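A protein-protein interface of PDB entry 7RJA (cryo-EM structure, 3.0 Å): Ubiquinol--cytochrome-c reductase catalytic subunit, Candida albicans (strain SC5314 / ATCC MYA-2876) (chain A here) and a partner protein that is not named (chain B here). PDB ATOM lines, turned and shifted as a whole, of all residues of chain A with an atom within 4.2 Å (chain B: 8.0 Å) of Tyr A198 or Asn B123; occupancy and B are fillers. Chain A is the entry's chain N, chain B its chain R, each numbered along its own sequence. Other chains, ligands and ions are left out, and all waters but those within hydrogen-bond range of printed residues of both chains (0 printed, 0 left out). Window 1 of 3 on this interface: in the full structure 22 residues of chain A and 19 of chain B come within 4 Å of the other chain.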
ATOM      1  N   LEU A  50      30.676  -9.771  -4.063  1.00  0.00           N
ATOM      2  CA  LEU A  50      30.305  -8.467  -4.587  1.00  0.00           C
ATOM      3  C   LEU A  50      28.863  -8.154  -4.220  1.00  0.00           C
ATOM      4  O   LEU A  50      27.968  -8.982  -4.403  1.00  0.00           O
ATOM      5  CB  LEU A  50      30.488  -8.442  -6.103  1.00  0.00           C
ATOM      6  CG  LEU A  50      30.030  -7.173  -6.817  1.00  0.00           C
ATOM      7  CD1 LEU A  50      30.759  -5.963  -6.280  1.00  0.00           C
ATOM      8  CD2 LEU A  50      30.253  -7.306  -8.308  1.00  0.00           C
ATOM      9  N   PRO A  52      25.292  -7.181  -4.492  1.00  0.00           N
ATOM     10  CA  PRO A  52      24.388  -7.028  -5.627  1.00  0.00           C
ATOM     11  C   PRO A  52      23.735  -5.659  -5.613  1.00  0.00           C
ATOM     12  O   PRO A  52      23.444  -5.117  -4.537  1.00  0.00           O
ATOM     13  CB  PRO A  52      23.357  -8.142  -5.410  1.00  0.00           C
ATOM     14  CG  PRO A  52      23.353  -8.355  -3.957  1.00  0.00           C
ATOM     15  CD  PRO A  52      24.764  -8.141  -3.507  1.00  0.00           C
ATOM     16  N   PRO A  53      23.478  -5.070  -6.777  1.00  0.00           N
ATOM     17  CA  PRO A  53      22.837  -3.752  -6.798  1.00  0.00           C
ATOM     18  C   PRO A  53      21.359  -3.832  -6.466  1.00  0.00           C
ATOM     19  O   PRO A  53      20.845  -4.911  -6.156  1.00  0.00           O
ATOM     20  CB  PRO A  53      23.073  -3.281  -8.233  1.00  0.00           C
ATOM     21  CG  PRO A  53      23.086  -4.534  -9.013  1.00  0.00           C
ATOM     22  CD  PRO A  53      23.752  -5.559  -8.138  1.00  0.00           C
ATOM     23  N   TYR A 171      20.232 -10.424  -5.182  1.00  0.00           N
ATOM     24  CA  TYR A 171      21.327 -11.384  -5.175  1.00  0.00           C
ATOM     25  C   TYR A 171      21.070 -12.504  -6.168  1.00  0.00           C
ATOM     26  O   TYR A 171      21.895 -12.768  -7.050  1.00  0.00           O
ATOM     27  CB  TYR A 171      21.509 -11.946  -3.768  1.00  0.00           C
ATOM     28  CG  TYR A 171      22.447 -13.119  -3.693  1.00  0.00           C
ATOM     29  CD1 TYR A 171      23.816 -12.942  -3.790  1.00  0.00           C
ATOM     30  CD2 TYR A 171      21.964 -14.403  -3.514  1.00  0.00           C
ATOM     31  CE1 TYR A 171      24.673 -14.011  -3.718  1.00  0.00           C
ATOM     32  CE2 TYR A 171      22.815 -15.477  -3.440  1.00  0.00           C
ATOM     33  CZ  TYR A 171      24.168 -15.276  -3.543  1.00  0.00           C
ATOM     34  OH  TYR A 171      25.023 -16.345  -3.472  1.00  0.00           O
ATOM     35  N   SER A 174      21.496 -11.199  -9.531  1.00  0.00           N
ATOM     36  CA  SER A 174      22.905 -10.917  -9.758  1.00  0.00           C
ATOM     37  C   SER A 174      23.704 -12.205  -9.842  1.00  0.00           C
ATOM     38  O   SER A 174      24.706 -12.278 -10.561  1.00  0.00           O
ATOM     39  CB  SER A 174      23.443 -10.020  -8.650  1.00  0.00           C
ATOM     40  OG  SER A 174      22.703  -8.816  -8.579  1.00  0.00           O
ATOM     41  N   GLY A 178      25.610 -12.939 -13.308  1.00  0.00           N
ATOM     42  CA  GLY A 178      26.889 -12.401 -12.894  1.00  0.00           C
ATOM     43  C   GLY A 178      28.076 -13.159 -13.447  1.00  0.00           C
ATOM     44  O   GLY A 178      29.213 -12.690 -13.349  1.00  0.00           O
ATOM     45  N   ASN A 196      31.867 -16.766 -10.065  1.00  0.00           N
ATOM     46  CA  ASN A 196      30.762 -15.822 -10.025  1.00  0.00           C
ATOM     47  C   ASN A 196      31.023 -14.814  -8.914  1.00  0.00           C
ATOM     48  O   ASN A 196      30.958 -15.173  -7.732  1.00  0.00           O
ATOM     49  CB  ASN A 196      29.435 -16.539  -9.793  1.00  0.00           C
ATOM     50  CG  ASN A 196      28.251 -15.618  -9.946  1.00  0.00           C
ATOM     51  OD1 ASN A 196      28.410 -14.405 -10.057  1.00  0.00           O
ATOM     52  ND2 ASN A 196      27.054 -16.186  -9.955  1.00  0.00           N
ATOM     53  N   PRO A 197      31.313 -13.551  -9.236  1.00  0.00           N
ATOM     54  CA  PRO A 197      31.740 -12.621  -8.182  1.00  0.00           C
ATOM     55  C   PRO A 197      30.722 -12.457  -7.073  1.00  0.00           C
ATOM     56  O   PRO A 197      31.109 -12.271  -5.912  1.00  0.00           O
ATOM     57  CB  PRO A 197      31.963 -11.309  -8.946  1.00  0.00           C
ATOM     58  CG  PRO A 197      31.108 -11.423 -10.143  1.00  0.00           C
ATOM     59  CD  PRO A 197      31.145 -12.866 -10.527  1.00  0.00           C
ATOM     60  N   TYR A 198      29.430 -12.529  -7.388  1.00  0.00           N
ATOM     61  CA  TYR A 198      28.406 -12.337  -6.372  1.00  0.00           C
ATOM     62  C   TYR A 198      28.327 -13.490  -5.386  1.00  0.00           C
ATOM     63  O   TYR A 198      27.652 -13.357  -4.362  1.00  0.00           O
ATOM     64  CB  TYR A 198      27.051 -12.127  -7.040  1.00  0.00           C
ATOM     65  CG  TYR A 198      27.033 -10.936  -7.962  1.00  0.00           C
ATOM     66  CD1 TYR A 198      26.816  -9.662  -7.471  1.00  0.00           C
ATOM     67  CD2 TYR A 198      27.247 -11.084  -9.320  1.00  0.00           C
ATOM     68  CE1 TYR A 198      26.804  -8.570  -8.307  1.00  0.00           C
ATOM     69  CE2 TYR A 198      27.237  -9.998 -10.165  1.00  0.00           C
ATOM     70  CZ  TYR A 198      27.015  -8.744  -9.652  1.00  0.00           C
ATOM     71  OH  TYR A 198      27.006  -7.658 -10.492  1.00  0.00           O
ATOM     72  N   PHE A 199      28.989 -14.601  -5.659  1.00  0.00           N
ATOM     73  CA  PHE A 199      29.014 -15.706  -4.709  1.00  0.00           C
ATOM     74  C   PHE A 199      30.138 -15.499  -3.701  1.00  0.00           C
ATOM     75  O   PHE A 199      31.276 -15.239  -4.101  1.00  0.00           O
ATOM     76  CB  PHE A 199      29.207 -17.031  -5.426  1.00  0.00           C
ATOM     77  CG  PHE A 199      29.039 -18.222  -4.538  1.00  0.00           C
ATOM     78  CD1 PHE A 199      27.792 -18.587  -4.076  1.00  0.00           C
ATOM     79  CD2 PHE A 199      30.131 -18.974  -4.160  1.00  0.00           C
ATOM     80  CE1 PHE A 199      27.642 -19.681  -3.257  1.00  0.00           C
ATOM     81  CE2 PHE A 199      29.985 -20.067  -3.342  1.00  0.00           C
ATOM     82  CZ  PHE A 199      28.739 -20.421  -2.891  1.00  0.00           C
ATOM     83  N   PRO A 200      29.867 -15.602  -2.402  1.00  0.00           N
ATOM     84  CA  PRO A 200      30.948 -15.462  -1.421  1.00  0.00           C
ATOM     85  C   PRO A 200      32.107 -16.390  -1.742  1.00  0.00           C
ATOM     86  O   PRO A 200      31.930 -17.593  -1.941  1.00  0.00           O
ATOM     87  CB  PRO A 200      30.272 -15.832  -0.099  1.00  0.00           C
ATOM     88  CG  PRO A 200      28.842 -15.536  -0.312  1.00  0.00           C
ATOM     89  CD  PRO A 200      28.565 -15.822  -1.752  1.00  0.00           C
ATOM     90  N   LEU B  66      20.582  -6.731 -20.733  1.00  0.00           N
ATOM     91  CA  LEU B  66      21.634  -6.586 -19.732  1.00  0.00           C
ATOM     92  C   LEU B  66      23.010  -6.482 -20.378  1.00  0.00           C
ATOM     93  O   LEU B  66      23.841  -5.676 -19.947  1.00  0.00           O
ATOM     94  CB  LEU B  66      21.596  -7.753 -18.751  1.00  0.00           C
ATOM     95  CG  LEU B  66      22.615  -7.702 -17.615  1.00  0.00           C
ATOM     96  CD1 LEU B  66      22.356  -6.511 -16.717  1.00  0.00           C
ATOM     97  CD2 LEU B  66      22.554  -8.987 -16.820  1.00  0.00           C
ATOM     98  N   ARG B  70      25.419  -3.280 -20.070  1.00  0.00           N
ATOM     99  CA  ARG B  70      26.778  -3.374 -19.553  1.00  0.00           C
ATOM    100  C   ARG B  70      27.769  -2.751 -20.522  1.00  0.00           C
ATOM    101  O   ARG B  70      28.660  -1.996 -20.116  1.00  0.00           O
ATOM    102  CB  ARG B  70      27.150  -4.831 -19.291  1.00  0.00           C
ATOM    103  CG  ARG B  70      26.989  -5.271 -17.851  1.00  0.00           C
ATOM    104  CD  ARG B  70      26.778  -6.771 -17.761  1.00  0.00           C
ATOM    105  NE  ARG B  70      26.395  -7.195 -16.421  1.00  0.00           N
ATOM    106  CZ  ARG B  70      26.002  -8.423 -16.111  1.00  0.00           C
ATOM    107  NH1 ARG B  70      25.943  -9.381 -17.021  1.00  0.00           N
ATOM    108  NH2 ARG B  70      25.665  -8.698 -14.855  1.00  0.00           N
ATOM    109  N   CYS B  73      27.503   0.995 -20.338  1.00  0.00           N
ATOM    110  CA  CYS B  73      27.978   1.586 -19.092  1.00  0.00           C
ATOM    111  C   CYS B  73      29.499   1.543 -19.000  1.00  0.00           C
ATOM    112  O   CYS B  73      30.130   2.521 -18.583  1.00  0.00           O
ATOM    113  CB  CYS B  73      27.340   0.871 -17.905  1.00  0.00           C
ATOM    114  SG  CYS B  73      25.554   1.105 -17.816  1.00  0.00           S
ATOM    115  N   THR B  74      30.111   0.421 -19.385  1.00  0.00           N
ATOM    116  CA  THR B  74      31.568   0.346 -19.357  1.00  0.00           C
ATOM    117  C   THR B  74      32.207   1.375 -20.275  1.00  0.00           C
ATOM    118  O   THR B  74      33.340   1.796 -20.022  1.00  0.00           O
ATOM    119  CB  THR B  74      32.052  -1.051 -19.747  1.00  0.00           C
ATOM    120  OG1 THR B  74      31.748  -1.296 -21.125  1.00  0.00           O
ATOM    121  CG2 THR B  74      31.425  -2.123 -18.864  1.00  0.00           C
ATOM    122  N   CYS B  79      32.960   4.942 -15.840  1.00  0.00           N
ATOM    123  CA  CYS B  79      33.477   3.579 -15.830  1.00  0.00           C
ATOM    124  C   CYS B  79      34.789   3.431 -16.587  1.00  0.00           C
ATOM    125  O   CYS B  79      35.448   2.395 -16.448  1.00  0.00           O
ATOM    126  CB  CYS B  79      32.449   2.621 -16.431  1.00  0.00           C
ATOM    127  SG  CYS B  79      30.928   2.461 -15.479  1.00  0.00           S
ATOM    128  N   PHE B 115      38.297  -5.979 -10.898  1.00  0.00           N
ATOM    129  CA  PHE B 115      37.039  -6.469 -11.443  1.00  0.00           C
ATOM    130  C   PHE B 115      35.871  -6.052 -10.568  1.00  0.00           C
ATOM    131  O   PHE B 115      34.811  -5.675 -11.074  1.00  0.00           O
ATOM    132  CB  PHE B 115      37.078  -7.988 -11.579  1.00  0.00           C
ATOM    133  CG  PHE B 115      35.853  -8.565 -12.217  1.00  0.00           C
ATOM    134  CD1 PHE B 115      35.465  -8.170 -13.482  1.00  0.00           C
ATOM    135  CD2 PHE B 115      35.084  -9.495 -11.547  1.00  0.00           C
ATOM    136  CE1 PHE B 115      34.338  -8.696 -14.070  1.00  0.00           C
ATOM    137  CE2 PHE B 115      33.956 -10.025 -12.130  1.00  0.00           C
ATOM    138  CZ  PHE B 115      33.583  -9.624 -13.394  1.00  0.00           C
ATOM    139  N   PHE B 116      36.041  -6.123  -9.247  1.00  0.00           N
ATOM    140  CA  PHE B 116      34.969  -5.728  -8.342  1.00  0.00           C
ATOM    141  C   PHE B 116      34.659  -4.247  -8.474  1.00  0.00           C
ATOM    142  O   PHE B 116      33.491  -3.848  -8.485  1.00  0.00           O
ATOM    143  CB  PHE B 116      35.348  -6.074  -6.906  1.00  0.00           C
ATOM    144  CG  PHE B 116      34.972  -7.466  -6.504  1.00  0.00           C
ATOM    145  CD1 PHE B 116      35.206  -8.529  -7.351  1.00  0.00           C
ATOM    146  CD2 PHE B 116      34.388  -7.710  -5.277  1.00  0.00           C
ATOM    147  CE1 PHE B 116      34.861  -9.807  -6.987  1.00  0.00           C
ATOM    148  CE2 PHE B 116      34.041  -8.988  -4.908  1.00  0.00           C
ATOM    149  CZ  PHE B 116      34.278 -10.039  -5.764  1.00  0.00           C
ATOM    150  N   HIS B 117      35.692  -3.412  -8.569  1.00  0.00           N
ATOM    151  CA  HIS B 117      35.455  -1.982  -8.742  1.00  0.00           C
ATOM    152  C   HIS B 117      34.715  -1.709 -10.045  1.00  0.00           C
ATOM    153  O   HIS B 117      33.740  -0.945 -10.075  1.00  0.00           O
ATOM    154  CB  HIS B 117      36.779  -1.223  -8.701  1.00  0.00           C
ATOM    155  CG  HIS B 117      37.443  -1.244  -7.362  1.00  0.00           C
ATOM    156  ND1 HIS B 117      38.720  -0.768  -7.157  1.00  0.00           N
ATOM    157  CD2 HIS B 117      37.008  -1.685  -6.158  1.00  0.00           C
ATOM    158  CE1 HIS B 117      39.042  -0.914  -5.884  1.00  0.00           C
ATOM    159  NE2 HIS B 117      38.020  -1.469  -5.257  1.00  0.00           N
ATOM    160  N   LEU B 118      35.160  -2.337 -11.135  1.00  0.00           N
ATOM    161  CA  LEU B 118      34.496  -2.140 -12.419  1.00  0.00           C
ATOM    162  C   LEU B 118      33.048  -2.598 -12.355  1.00  0.00           C
ATOM    163  O   LEU B 118      32.144  -1.911 -12.844  1.00  0.00           O
ATOM    164  CB  LEU B 118      35.243  -2.891 -13.519  1.00  0.00           C
ATOM    165  CG  LEU B 118      34.526  -2.971 -14.867  1.00  0.00           C
ATOM    166  CD1 LEU B 118      34.288  -1.583 -15.421  1.00  0.00           C
ATOM    167  CD2 LEU B 118      35.328  -3.804 -15.845  1.00  0.00           C
ATOM    168  N   GLN B 119      32.808  -3.763 -11.757  1.00  0.00           N
ATOM    169  CA  GLN B 119      31.455  -4.292 -11.693  1.00  0.00           C
ATOM    170  C   GLN B 119      30.559  -3.430 -10.823  1.00  0.00           C
ATOM    171  O   GLN B 119      29.386  -3.248 -11.150  1.00  0.00           O
ATOM    172  CB  GLN B 119      31.477  -5.729 -11.177  1.00  0.00           C
ATOM    173  CG  GLN B 119      31.839  -6.752 -12.235  1.00  0.00           C
ATOM    174  CD  GLN B 119      30.910  -6.706 -13.425  1.00  0.00           C
ATOM    175  OE1 GLN B 119      29.703  -6.539 -13.273  1.00  0.00           O
ATOM    176  NE2 GLN B 119      31.470  -6.842 -14.619  1.00  0.00           N
ATOM    177  N   HIS B 120      31.074  -2.895  -9.717  1.00  0.00           N
ATOM    178  CA  HIS B 120      30.262  -1.996  -8.907  1.00  0.00           C
ATOM    179  C   HIS B 120      29.923  -0.727  -9.675  1.00  0.00           C
ATOM    180  O   HIS B 120      28.772  -0.268  -9.656  1.00  0.00           O
ATOM    181  CB  HIS B 120      30.984  -1.657  -7.607  1.00  0.00           C
ATOM    182  CG  HIS B 120      30.119  -0.962  -6.605  1.00  0.00           C
ATOM    183  ND1 HIS B 120      29.112  -1.604  -5.920  1.00  0.00           N
ATOM    184  CD2 HIS B 120      30.104   0.323  -6.178  1.00  0.00           C
ATOM    185  CE1 HIS B 120      28.517  -0.748  -5.110  1.00  0.00           C
ATOM    186  NE2 HIS B 120      29.101   0.429  -5.247  1.00  0.00           N
ATOM    187  N   CYS B 121      30.907  -0.149 -10.366  1.00  0.00           N
ATOM    188  CA  CYS B 121      30.644   1.067 -11.123  1.00  0.00           C
ATOM    189  C   CYS B 121      29.685   0.819 -12.279  1.00  0.00           C
ATOM    190  O   CYS B 121      28.944   1.730 -12.660  1.00  0.00           O
ATOM    191  CB  CYS B 121      31.954   1.652 -11.648  1.00  0.00           C
ATOM    192  SG  CYS B 121      31.800   3.329 -12.299  1.00  0.00           S
ATOM    193  N   VAL B 122      29.682  -0.389 -12.841  1.00  0.00           N
ATOM    194  CA  VAL B 122      28.757  -0.710 -13.923  1.00  0.00           C
ATOM    195  C   VAL B 122      27.370  -1.014 -13.376  1.00  0.00           C
ATOM    196  O   VAL B 122      26.358  -0.679 -13.999  1.00  0.00           O
ATOM    197  CB  VAL B 122      29.307  -1.885 -14.748  1.00  0.00           C
ATOM    198  CG1 VAL B 122      28.243  -2.423 -15.683  1.00  0.00           C
ATOM    199  CG2 VAL B 122      30.525  -1.446 -15.531  1.00  0.00           C
ATOM    200  N   ASN B 123      27.302  -1.676 -12.222  1.00  0.00           N
ATOM    201  CA  ASN B 123      26.015  -1.989 -11.621  1.00  0.00           C
ATOM    202  C   ASN B 123      25.291  -0.722 -11.196  1.00  0.00           C
ATOM    203  O   ASN B 123      24.079  -0.591 -11.404  1.00  0.00           O
ATOM    204  CB  ASN B 123      26.215  -2.926 -10.436  1.00  0.00           C
ATOM    205  CG  ASN B 123      26.369  -4.367 -10.860  1.00  0.00           C
ATOM    206  OD1 ASN B 123      26.192  -4.702 -12.031  1.00  0.00           O
ATOM    207  ND2 ASN B 123      26.705  -5.231  -9.913  1.00  0.00           N
ATOM    208  N   ASP B 124      26.023   0.242 -10.632  1.00  0.00           N
ATOM    209  CA  ASP B 124      25.384   1.490 -10.235  1.00  0.00           C
ATOM    210  C   ASP B 124      24.712   2.178 -11.411  1.00  0.00           C
ATOM    211  O   ASP B 124      23.818   3.005 -11.204  1.00  0.00           O
ATOM    212  CB  ASP B 124      26.405   2.435  -9.602  1.00  0.00           C
ATOM    213  CG  ASP B 124      26.894   1.947  -8.259  1.00  0.00           C
ATOM    214  OD1 ASP B 124      26.125   1.251  -7.564  1.00  0.00           O
ATOM    215  OD2 ASP B 124      28.046   2.261  -7.894  1.00  0.00           O
ATOM    216  N   CYS B 125      25.121   1.857 -12.637  1.00  0.00           N
ATOM    217  CA  CYS B 125      24.490   2.415 -13.824  1.00  0.00           C
ATOM    218  C   CYS B 125      23.376   1.523 -14.359  1.00  0.00           C
ATOM    219  O   CYS B 125      22.295   2.020 -14.687  1.00  0.00           O
ATOM    220  CB  CYS B 125      25.538   2.640 -14.914  1.00  0.00           C
ATOM    221  SG  CYS B 125      26.778   3.890 -14.511  1.00  0.00           S
ATOM    222  N   VAL B 126      23.611   0.213 -14.452  1.00  0.00           N
ATOM    223  CA  VAL B 126      22.620  -0.663 -15.073  1.00  0.00           C
ATOM    224  C   VAL B 126      21.386  -0.799 -14.191  1.00  0.00           C
ATOM    225  O   VAL B 126      20.257  -0.852 -14.693  1.00  0.00           O
ATOM    226  CB  VAL B 126      23.222  -2.043 -15.395  1.00  0.00           C
ATOM    227  CG1 VAL B 126      24.450  -1.909 -16.274  1.00  0.00           C
ATOM    228  CG2 VAL B 126      23.529  -2.798 -14.124  1.00  0.00           C
ATOM    229  N   ALA B 127      21.571  -0.868 -12.869  1.00  0.00           N
ATOM    230  CA  ALA B 127      20.487  -1.182 -11.947  1.00  0.00           C
ATOM    231  C   ALA B 127      19.217  -0.397 -12.252  1.00  0.00           C
ATOM    232  O   ALA B 127      18.185  -1.003 -12.564  1.00  0.00           O
ATOM    233  CB  ALA B 127      20.932  -0.922 -10.507  1.00  0.00           C
ATOM    234  N   PRO B 128      19.234   0.936 -12.179  1.00  0.00           N
ATOM    235  CA  PRO B 128      17.984   1.686 -12.384  1.00  0.00           C
ATOM    236  C   PRO B 128      17.372   1.498 -13.758  1.00  0.00           C
ATOM    237  O   PRO B 128      16.144   1.576 -13.887  1.00  0.00           O
ATOM    238  CB  PRO B 128      18.409   3.142 -12.154  1.00  0.00           C
ATOM    239  CG  PRO B 128      19.854   3.160 -12.471  1.00  0.00           C
ATOM    240  CD  PRO B 128      20.383   1.840 -12.001  1.00  0.00           C
ATOM    241  N   ARG B 129      18.177   1.250 -14.789  1.00  0.00           N
ATOM    242  CA  ARG B 129      17.679   1.213 -16.156  1.00  0.00           C
ATOM    243  C   ARG B 129      17.312  -0.181 -16.640  1.00  0.00           C
ATOM    244  O   ARG B 129      16.582  -0.297 -17.629  1.00  0.00           O
ATOM    245  CB  ARG B 129      18.725   1.794 -17.115  1.00  0.00           C
ATOM    246  CG  ARG B 129      19.165   3.214 -16.795  1.00  0.00           C
ATOM    247  CD  ARG B 129      20.633   3.415 -17.125  1.00  0.00           C
ATOM    248  NE  ARG B 129      20.908   3.214 -18.542  1.00  0.00           N
ATOM    249  CZ  ARG B 129      20.543   4.048 -19.506  1.00  0.00           C
ATOM    250  NH1 ARG B 129      19.887   5.165 -19.242  1.00  0.00           N
ATOM    251  NH2 ARG B 129      20.845   3.752 -20.766  1.00  0.00           N
ATOM    252  N   LEU B 130      17.788  -1.234 -15.979  1.00  0.00           N
ATOM    253  CA  LEU B 130      17.661  -2.575 -16.538  1.00  0.00           C
ATOM    254  C   LEU B 130      16.199  -2.974 -16.709  1.00  0.00           C
ATOM    255  O   LEU B 130      15.777  -3.379 -17.797  1.00  0.00           O
ATOM    256  CB  LEU B 130      18.391  -3.581 -15.650  1.00  0.00           C
ATOM    257  CG  LEU B 130      18.310  -5.037 -16.105  1.00  0.00           C
ATOM    258  CD1 LEU B 130      18.919  -5.208 -17.481  1.00  0.00           C
ATOM    259  CD2 LEU B 130      18.999  -5.938 -15.103  1.00  0.00           C
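Printed residues of chain B within 4 Å of Leu A50: Phe B116 and Gln B119. Of chain B, only Asn B123 (2.5 Å) comes within 4 Å of Tyr A198. Of the printed residues of chain A, Phe B115 touches Pro A197 (3.7 Å). Val B122 touches none of the printed residues of chain A. Asn B123 touches just these residues of chain A: Pro A53 and Tyr A198. Cys B125 touches none of the printed residues of chain A. The nearest residue of chain B that does not touch Tyr A198 is Gln B119 (4.03 Å). The nearest printed residue of chain A that does not touch Asn B123 is Leu A50 (4.4 Å).
The side-chain amide oxygen of Asn A196 sits close to the backbone NH of Tyr A198 (3.4 Å). The backbone NH (N) of Leu A50 is in hydrogen-bond range of the backbone carbonyl oxygen (O) of Pro A197 (3.1 Å).
Phe B116 touches Leu A50 (CE2 to N, 3.6 Å). Gln B119 touches Leu A50. CD of Pro A53 touches ND2 of Asn B123, 3.5 Å away. Ala B127 touches Pro A53 (CB to CB, 3.9 Å). Phe B115 touches Pro A197 (CE2 to CG, 3.7 Å). Pro A197 touches Phe B116.
OH of Tyr A198 sits at hydrogen-bond distance from ND2 of Asn B123, at 2.5 Å.
Of the 11 printed residues of chain A, 4 touch a printed residue of chain B. Hydrophobic or aromatic side chains of chain A within 4 Å of the printed part of chain B: Leu A50, Pro A53, Pro A197 and Tyr A198. Along chain A the printed residues that touch a printed residue of chain B span positions 50 to 198. Among the printed residues, no Asp or Glu carboxylate lies within 4 Å of a Lys or Arg side-chain nitrogen of the other chain.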
